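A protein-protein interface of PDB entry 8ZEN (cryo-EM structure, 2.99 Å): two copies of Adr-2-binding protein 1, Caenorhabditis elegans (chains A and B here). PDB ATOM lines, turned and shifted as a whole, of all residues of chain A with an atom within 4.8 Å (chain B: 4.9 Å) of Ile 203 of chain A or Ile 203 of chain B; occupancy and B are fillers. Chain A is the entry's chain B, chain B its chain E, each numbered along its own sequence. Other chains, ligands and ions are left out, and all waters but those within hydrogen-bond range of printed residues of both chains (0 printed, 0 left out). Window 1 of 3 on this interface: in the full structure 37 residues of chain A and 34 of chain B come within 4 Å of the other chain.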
ATOM      1  N   TYR A 180     -22.700  -3.581  25.535  1.00  0.00           N
ATOM      2  CA  TYR A 180     -23.315  -4.893  25.371  1.00  0.00           C
ATOM      3  C   TYR A 180     -22.282  -5.929  24.954  1.00  0.00           C
ATOM      4  O   TYR A 180     -22.297  -7.067  25.435  1.00  0.00           O
ATOM      5  CB  TYR A 180     -24.448  -4.830  24.349  1.00  0.00           C
ATOM      6  CG  TYR A 180     -25.230  -6.118  24.264  1.00  0.00           C
ATOM      7  CD1 TYR A 180     -26.245  -6.390  25.167  1.00  0.00           C
ATOM      8  CD2 TYR A 180     -24.941  -7.070  23.299  1.00  0.00           C
ATOM      9  CE1 TYR A 180     -26.960  -7.565  25.105  1.00  0.00           C
ATOM     10  CE2 TYR A 180     -25.650  -8.251  23.230  1.00  0.00           C
ATOM     11  CZ  TYR A 180     -26.658  -8.493  24.136  1.00  0.00           C
ATOM     12  OH  TYR A 180     -27.377  -9.664  24.077  1.00  0.00           O
ATOM     13  N   VAL A 184     -21.169  -9.325  26.860  1.00  0.00           N
ATOM     14  CA  VAL A 184     -21.117 -10.626  26.195  1.00  0.00           C
ATOM     15  C   VAL A 184     -19.743 -11.258  26.376  1.00  0.00           C
ATOM     16  O   VAL A 184     -19.624 -12.458  26.641  1.00  0.00           O
ATOM     17  CB  VAL A 184     -21.480 -10.484  24.707  1.00  0.00           C
ATOM     18  CG1 VAL A 184     -21.190 -11.772  23.963  1.00  0.00           C
ATOM     19  CG2 VAL A 184     -22.939 -10.109  24.558  1.00  0.00           C
ATOM     20  N   LEU A 188     -18.825 -14.717  28.249  1.00  0.00           N
ATOM     21  CA  LEU A 188     -18.051 -15.767  27.596  1.00  0.00           C
ATOM     22  C   LEU A 188     -16.793 -16.109  28.382  1.00  0.00           C
ATOM     23  O   LEU A 188     -16.402 -17.279  28.447  1.00  0.00           O
ATOM     24  CB  LEU A 188     -17.688 -15.342  26.174  1.00  0.00           C
ATOM     25  CG  LEU A 188     -18.599 -15.771  25.022  1.00  0.00           C
ATOM     26  CD1 LEU A 188     -18.595 -17.278  24.870  1.00  0.00           C
ATOM     27  CD2 LEU A 188     -20.015 -15.267  25.225  1.00  0.00           C
ATOM     28  N   ILE A 199     -22.124 -21.229  22.997  1.00  0.00           N
ATOM     29  CA  ILE A 199     -22.655 -19.870  22.921  1.00  0.00           C
ATOM     30  C   ILE A 199     -22.105 -19.157  21.695  1.00  0.00           C
ATOM     31  O   ILE A 199     -22.820 -18.408  21.021  1.00  0.00           O
ATOM     32  CB  ILE A 199     -22.340 -19.087  24.210  1.00  0.00           C
ATOM     33  CG1 ILE A 199     -23.156 -19.619  25.381  1.00  0.00           C
ATOM     34  CG2 ILE A 199     -22.625 -17.609  24.021  1.00  0.00           C
ATOM     35  CD1 ILE A 199     -22.886 -18.907  26.684  1.00  0.00           C
ATOM     36  N   THR A 200     -20.822 -19.369  21.395  1.00  0.00           N
ATOM     37  CA  THR A 200     -20.211 -18.728  20.235  1.00  0.00           C
ATOM     38  C   THR A 200     -20.889 -19.167  18.942  1.00  0.00           C
ATOM     39  O   THR A 200     -21.255 -18.330  18.105  1.00  0.00           O
ATOM     40  CB  THR A 200     -18.716 -19.039  20.199  1.00  0.00           C
ATOM     41  OG1 THR A 200     -18.022 -18.151  21.082  1.00  0.00           O
ATOM     42  CG2 THR A 200     -18.165 -18.877  18.792  1.00  0.00           C
ATOM     43  N   GLN A 201     -21.073 -20.479  18.761  1.00  0.00           N
ATOM     44  CA  GLN A 201     -21.757 -20.952  17.558  1.00  0.00           C
ATOM     45  C   GLN A 201     -23.193 -20.447  17.507  1.00  0.00           C
ATOM     46  O   GLN A 201     -23.695 -20.094  16.437  1.00  0.00           O
ATOM     47  CB  GLN A 201     -21.733 -22.479  17.431  1.00  0.00           C
ATOM     48  CG  GLN A 201     -20.396 -23.083  17.033  1.00  0.00           C
ATOM     49  CD  GLN A 201     -19.797 -23.968  18.096  1.00  0.00           C
ATOM     50  OE1 GLN A 201     -20.350 -24.117  19.180  1.00  0.00           O
ATOM     51  NE2 GLN A 201     -18.666 -24.586  17.780  1.00  0.00           N
ATOM     52  N   ALA A 202     -23.879 -20.418  18.651  1.00  0.00           N
ATOM     53  CA  ALA A 202     -25.258 -19.941  18.658  1.00  0.00           C
ATOM     54  C   ALA A 202     -25.342 -18.474  18.253  1.00  0.00           C
ATOM     55  O   ALA A 202     -26.220 -18.088  17.470  1.00  0.00           O
ATOM     56  CB  ALA A 202     -25.877 -20.157  20.038  1.00  0.00           C
ATOM     57  N   ILE A 203     -24.436 -17.643  18.775  1.00  0.00           N
ATOM     58  CA  ILE A 203     -24.434 -16.223  18.436  1.00  0.00           C
ATOM     59  C   ILE A 203     -24.111 -16.032  16.960  1.00  0.00           C
ATOM     60  O   ILE A 203     -24.747 -15.228  16.269  1.00  0.00           O
ATOM     61  CB  ILE A 203     -23.452 -15.452  19.334  1.00  0.00           C
ATOM     62  CG1 ILE A 203     -23.994 -15.350  20.759  1.00  0.00           C
ATOM     63  CG2 ILE A 203     -23.205 -14.061  18.785  1.00  0.00           C
ATOM     64  CD1 ILE A 203     -23.066 -14.626  21.707  1.00  0.00           C
ATOM     65  N   THR A 204     -23.122 -16.771  16.454  1.00  0.00           N
ATOM     66  CA  THR A 204     -22.808 -16.684  15.032  1.00  0.00           C
ATOM     67  C   THR A 204     -23.996 -17.113  14.178  1.00  0.00           C
ATOM     68  O   THR A 204     -24.278 -16.489  13.149  1.00  0.00           O
ATOM     69  CB  THR A 204     -21.575 -17.532  14.715  1.00  0.00           C
ATOM     70  OG1 THR A 204     -20.391 -16.798  15.050  1.00  0.00           O
ATOM     71  CG2 THR A 204     -21.529 -17.901  13.241  1.00  0.00           C
ATOM     72  N   ALA A 205     -24.715 -18.153  14.601  1.00  0.00           N
ATOM     73  CA  ALA A 205     -25.866 -18.625  13.842  1.00  0.00           C
ATOM     74  C   ALA A 205     -26.982 -17.588  13.817  1.00  0.00           C
ATOM     75  O   ALA A 205     -27.571 -17.327  12.763  1.00  0.00           O
ATOM     76  CB  ALA A 205     -26.372 -19.946  14.425  1.00  0.00           C
ATOM     77  N   THR A 206     -27.293 -16.984  14.969  1.00  0.00           N
ATOM     78  CA  THR A 206     -28.373 -15.999  14.974  1.00  0.00           C
ATOM     79  C   THR A 206     -27.960 -14.719  14.262  1.00  0.00           C
ATOM     80  O   THR A 206     -28.819 -13.998  13.741  1.00  0.00           O
ATOM     81  CB  THR A 206     -28.840 -15.676  16.394  1.00  0.00           C
ATOM     82  OG1 THR A 206     -29.679 -14.516  16.358  1.00  0.00           O
ATOM     83  CG2 THR A 206     -27.674 -15.374  17.292  1.00  0.00           C
ATOM     84  N   ILE A 207     -26.662 -14.412  14.232  1.00  0.00           N
ATOM     85  CA  ILE A 207     -26.194 -13.253  13.481  1.00  0.00           C
ATOM     86  C   ILE A 207     -26.304 -13.514  11.983  1.00  0.00           C
ATOM     87  O   ILE A 207     -26.758 -12.656  11.217  1.00  0.00           O
ATOM     88  CB  ILE A 207     -24.757 -12.896  13.898  1.00  0.00           C
ATOM     89  CG1 ILE A 207     -24.780 -11.908  15.063  1.00  0.00           C
ATOM     90  CG2 ILE A 207     -23.991 -12.299  12.735  1.00  0.00           C
ATOM     91  CD1 ILE A 207     -23.413 -11.571  15.599  1.00  0.00           C
ATOM     92  N   TYR B 180     -13.928 -11.789  19.542  1.00  0.00           N
ATOM     93  CA  TYR B 180     -15.319 -12.126  19.261  1.00  0.00           C
ATOM     94  C   TYR B 180     -16.251 -10.997  19.683  1.00  0.00           C
ATOM     95  O   TYR B 180     -17.196 -10.659  18.963  1.00  0.00           O
ATOM     96  CB  TYR B 180     -15.701 -13.429  19.958  1.00  0.00           C
ATOM     97  CG  TYR B 180     -16.983 -14.027  19.432  1.00  0.00           C
ATOM     98  CD1 TYR B 180     -16.995 -14.758  18.256  1.00  0.00           C
ATOM     99  CD2 TYR B 180     -18.182 -13.851  20.106  1.00  0.00           C
ATOM    100  CE1 TYR B 180     -18.160 -15.302  17.767  1.00  0.00           C
ATOM    101  CE2 TYR B 180     -19.354 -14.392  19.624  1.00  0.00           C
ATOM    102  CZ  TYR B 180     -19.337 -15.116  18.454  1.00  0.00           C
ATOM    103  OH  TYR B 180     -20.500 -15.662  17.965  1.00  0.00           O
ATOM    104  N   VAL B 184     -18.726  -8.809  17.355  1.00  0.00           N
ATOM    105  CA  VAL B 184     -20.146  -8.678  17.670  1.00  0.00           C
ATOM    106  C   VAL B 184     -20.545  -7.209  17.707  1.00  0.00           C
ATOM    107  O   VAL B 184     -21.581  -6.813  17.162  1.00  0.00           O
ATOM    108  CB  VAL B 184     -20.469  -9.388  18.996  1.00  0.00           C
ATOM    109  CG1 VAL B 184     -21.852  -9.009  19.482  1.00  0.00           C
ATOM    110  CG2 VAL B 184     -20.369 -10.890  18.824  1.00  0.00           C
ATOM    111  N   ILE B 199     -31.201  -8.781  16.963  1.00  0.00           N
ATOM    112  CA  ILE B 199     -29.955  -9.489  17.239  1.00  0.00           C
ATOM    113  C   ILE B 199     -29.668  -9.529  18.735  1.00  0.00           C
ATOM    114  O   ILE B 199     -29.218 -10.552  19.265  1.00  0.00           O
ATOM    115  CB  ILE B 199     -28.796  -8.854  16.452  1.00  0.00           C
ATOM    116  CG1 ILE B 199     -28.894  -9.232  14.975  1.00  0.00           C
ATOM    117  CG2 ILE B 199     -27.457  -9.301  17.010  1.00  0.00           C
ATOM    118  CD1 ILE B 199     -27.890  -8.527  14.098  1.00  0.00           C
ATOM    119  N   THR B 200     -29.913  -8.424  19.446  1.00  0.00           N
ATOM    120  CA  THR B 200     -29.385  -8.328  20.805  1.00  0.00           C
ATOM    121  C   THR B 200     -30.289  -9.029  21.825  1.00  0.00           C
ATOM    122  O   THR B 200     -29.782  -9.644  22.769  1.00  0.00           O
ATOM    123  CB  THR B 200     -29.096  -6.863  21.168  1.00  0.00           C
ATOM    124  OG1 THR B 200     -28.086  -6.812  22.179  1.00  0.00           O
ATOM    125  CG2 THR B 200     -30.301  -6.135  21.667  1.00  0.00           C
ATOM    126  N   GLN B 201     -31.617  -9.006  21.642  1.00  0.00           N
ATOM    127  CA  GLN B 201     -32.445  -9.941  22.410  1.00  0.00           C
ATOM    128  C   GLN B 201     -32.117 -11.389  22.068  1.00  0.00           C
ATOM    129  O   GLN B 201     -32.214 -12.267  22.929  1.00  0.00           O
ATOM    130  CB  GLN B 201     -33.953  -9.691  22.232  1.00  0.00           C
ATOM    131  CG  GLN B 201     -34.598  -8.420  22.837  1.00  0.00           C
ATOM    132  CD  GLN B 201     -34.040  -7.102  22.379  1.00  0.00           C
ATOM    133  OE1 GLN B 201     -33.018  -7.043  21.731  1.00  0.00           O
ATOM    134  NE2 GLN B 201     -34.724  -6.020  22.734  1.00  0.00           N
ATOM    135  N   ALA B 202     -31.732 -11.665  20.821  1.00  0.00           N
ATOM    136  CA  ALA B 202     -31.357 -13.033  20.471  1.00  0.00           C
ATOM    137  C   ALA B 202     -30.107 -13.472  21.226  1.00  0.00           C
ATOM    138  O   ALA B 202     -30.053 -14.589  21.756  1.00  0.00           O
ATOM    139  CB  ALA B 202     -31.144 -13.154  18.963  1.00  0.00           C
ATOM    140  N   ILE B 203     -29.099 -12.603  21.289  1.00  0.00           N
ATOM    141  CA  ILE B 203     -27.880 -12.918  22.030  1.00  0.00           C
ATOM    142  C   ILE B 203     -28.189 -13.041  23.517  1.00  0.00           C
ATOM    143  O   ILE B 203     -27.664 -13.921  24.211  1.00  0.00           O
ATOM    144  CB  ILE B 203     -26.800 -11.858  21.756  1.00  0.00           C
ATOM    145  CG1 ILE B 203     -26.342 -11.934  20.299  1.00  0.00           C
ATOM    146  CG2 ILE B 203     -25.615 -12.042  22.686  1.00  0.00           C
ATOM    147  CD1 ILE B 203     -25.341 -10.869  19.921  1.00  0.00           C
ATOM    148  N   THR B 204     -29.057 -12.163  24.026  1.00  0.00           N
ATOM    149  CA  THR B 204     -29.485 -12.258  25.418  1.00  0.00           C
ATOM    150  C   THR B 204     -30.129 -13.607  25.702  1.00  0.00           C
ATOM    151  O   THR B 204     -29.793 -14.273  26.687  1.00  0.00           O
ATOM    152  CB  THR B 204     -30.459 -11.124  25.737  1.00  0.00           C
ATOM    153  OG1 THR B 204     -29.827  -9.862  25.493  1.00  0.00           O
ATOM    154  CG2 THR B 204     -30.914 -11.199  27.185  1.00  0.00           C
ATOM    155  N   ALA B 205     -31.062 -14.027  24.845  1.00  0.00           N
ATOM    156  CA  ALA B 205     -31.744 -15.300  25.039  1.00  0.00           C
ATOM    157  C   ALA B 205     -30.775 -16.467  24.966  1.00  0.00           C
ATOM    158  O   ALA B 205     -30.875 -17.406  25.763  1.00  0.00           O
ATOM    159  CB  ALA B 205     -32.853 -15.466  24.001  1.00  0.00           C
ATOM    160  N   THR B 206     -29.832 -16.427  24.024  1.00  0.00           N
ATOM    161  CA  THR B 206     -28.825 -17.477  23.949  1.00  0.00           C
ATOM    162  C   THR B 206     -28.009 -17.542  25.234  1.00  0.00           C
ATOM    163  O   THR B 206     -27.725 -18.630  25.747  1.00  0.00           O
ATOM    164  CB  THR B 206     -27.916 -17.247  22.743  1.00  0.00           C
ATOM    165  OG1 THR B 206     -28.637 -17.540  21.541  1.00  0.00           O
ATOM    166  CG2 THR B 206     -26.687 -18.134  22.824  1.00  0.00           C
ATOM    167  N   ILE B 207     -27.632 -16.383  25.777  1.00  0.00           N
ATOM    168  CA  ILE B 207     -26.850 -16.365  27.010  1.00  0.00           C
ATOM    169  C   ILE B 207     -27.656 -16.953  28.163  1.00  0.00           C
ATOM    170  O   ILE B 207     -27.166 -17.803  28.916  1.00  0.00           O
ATOM    171  CB  ILE B 207     -26.370 -14.937  27.320  1.00  0.00           C
ATOM    172  CG1 ILE B 207     -25.265 -14.530  26.344  1.00  0.00           C
ATOM    173  CG2 ILE B 207     -25.885 -14.839  28.756  1.00  0.00           C
ATOM    174  CD1 ILE B 207     -24.475 -13.316  26.774  1.00  0.00           C
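O of Thr 200 of chain B lies within hydrogen-bond range of OG1 of Thr 204 of chain B, at 2.7 Å.
The backbone carbonyl oxygen of Ala 202 of chain B sits at hydrogen-bond distance from the side-chain hydroxyl of Thr 206 of chain B (3.3 Å).
Tyr 180 of chain A touches Thr 200 of chain B, and with the chains exchanged Thr 200 of chain A touches Tyr 180 of chain B.
Val 184 of chain A touches Ile 203 of chain B, but with the chains exchanged Ile 203 of chain A does not touch Val 184 of chain B (4.3 Å).
Ala 202 of chain A touches Thr 206 of chain B, and with the chains exchanged Thr 206 of chain A touches Ala 202 of chain B.
Ile 203 of chain B touches its own counterpart, Ile 203 of chain A.
Positions printed for both chains: 180, 184, 199, 200, 201, 202, 203, 204, 205, 206 and 207.
Tyr 180 of chain A touches Ile 203 of chain B (OH to CB, 3.2 Å).
Ile 203 of chain B touches Val 184 of chain A.
Ala 202 of chain A touches Thr 206 of chain B (CB to CG2, 3.5 Å).
CG2 of Ile 203 of chain A touches OH of Tyr 180 of chain B, 3.2 Å away.
Ile 203 of chain B touches Ile 203 of chain A.
Thr 206 of chain A touches Ala 202 of chain B (OG1 to CB, 3.3 Å).
Printed residues of chain B that touch a printed residue of chain A: Tyr 180, Thr 200, Ala 202, Ile 203, Thr 204 and Thr 206.
Of the 12 printed residues of chain A, 7 touch a printed residue of chain B.
Printed residues of chain A that touch a printed residue of chain B: Tyr 180, Val 184, Thr 200, Ala 202, Ile 203, Thr 204 and Thr 206.
Hydrophobic or aromatic side chains of chain A that line the printed part of chain B: Tyr 180, Val 184, Ala 202 and Ile 203.
Along chain A the printed residues that touch a printed residue of chain B span positions 180 to 206.
Among the printed residues, no Asp or Glu carboxylate lies within 4 Å of a Lys or Arg side-chain nitrogen of the other chain.
OH of Tyr 180 of chain A sits at hydrogen-bond distance from O of Thr 200 of chain B.
The side-chain hydroxyl (OG1) of Thr 204 of chain B lies within hydrogen-bond range of the side-chain hydroxyl (OH) of Tyr 180 of chain A (2.8 Å).
OH of Tyr 180 of chain B lies within hydrogen-bond range of O of Thr 200 of chain A (2.8 Å).
OH of Tyr 180 of chain B is in hydrogen-bond range of OG1 of Thr 204 of chain A.
Ile 203 of chain A touches just these residues of chain B: Tyr 180 (3.2 Å) and Ile 203 (3.8 Å).
Ile 203 of chain B touches just these residues of chain A: Tyr 180, Val 184 and Ile 203.
Of the printed residues of chain B, Val 184 of chain A touches Ile 203.
Of the printed residues of chain B, Thr 200 of chain A touches Tyr 180 (2.8 Å).
Printed residues of chain B within 4 Å of Ala 202 of chain A: Thr 206 (3.5 Å).
Of the printed residues of chain A, Thr 204 of chain B touches Tyr 180.
Printed residues of chain B within 4 Å of Thr 204 of chain A: Tyr 180 (3.1 Å).
Ile 207 of chain B touches none of the printed residues of chain A.
The nearest printed residue of chain A that does not touch Ile 203 of chain B is Thr 206 of chain A (4.8 Å).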
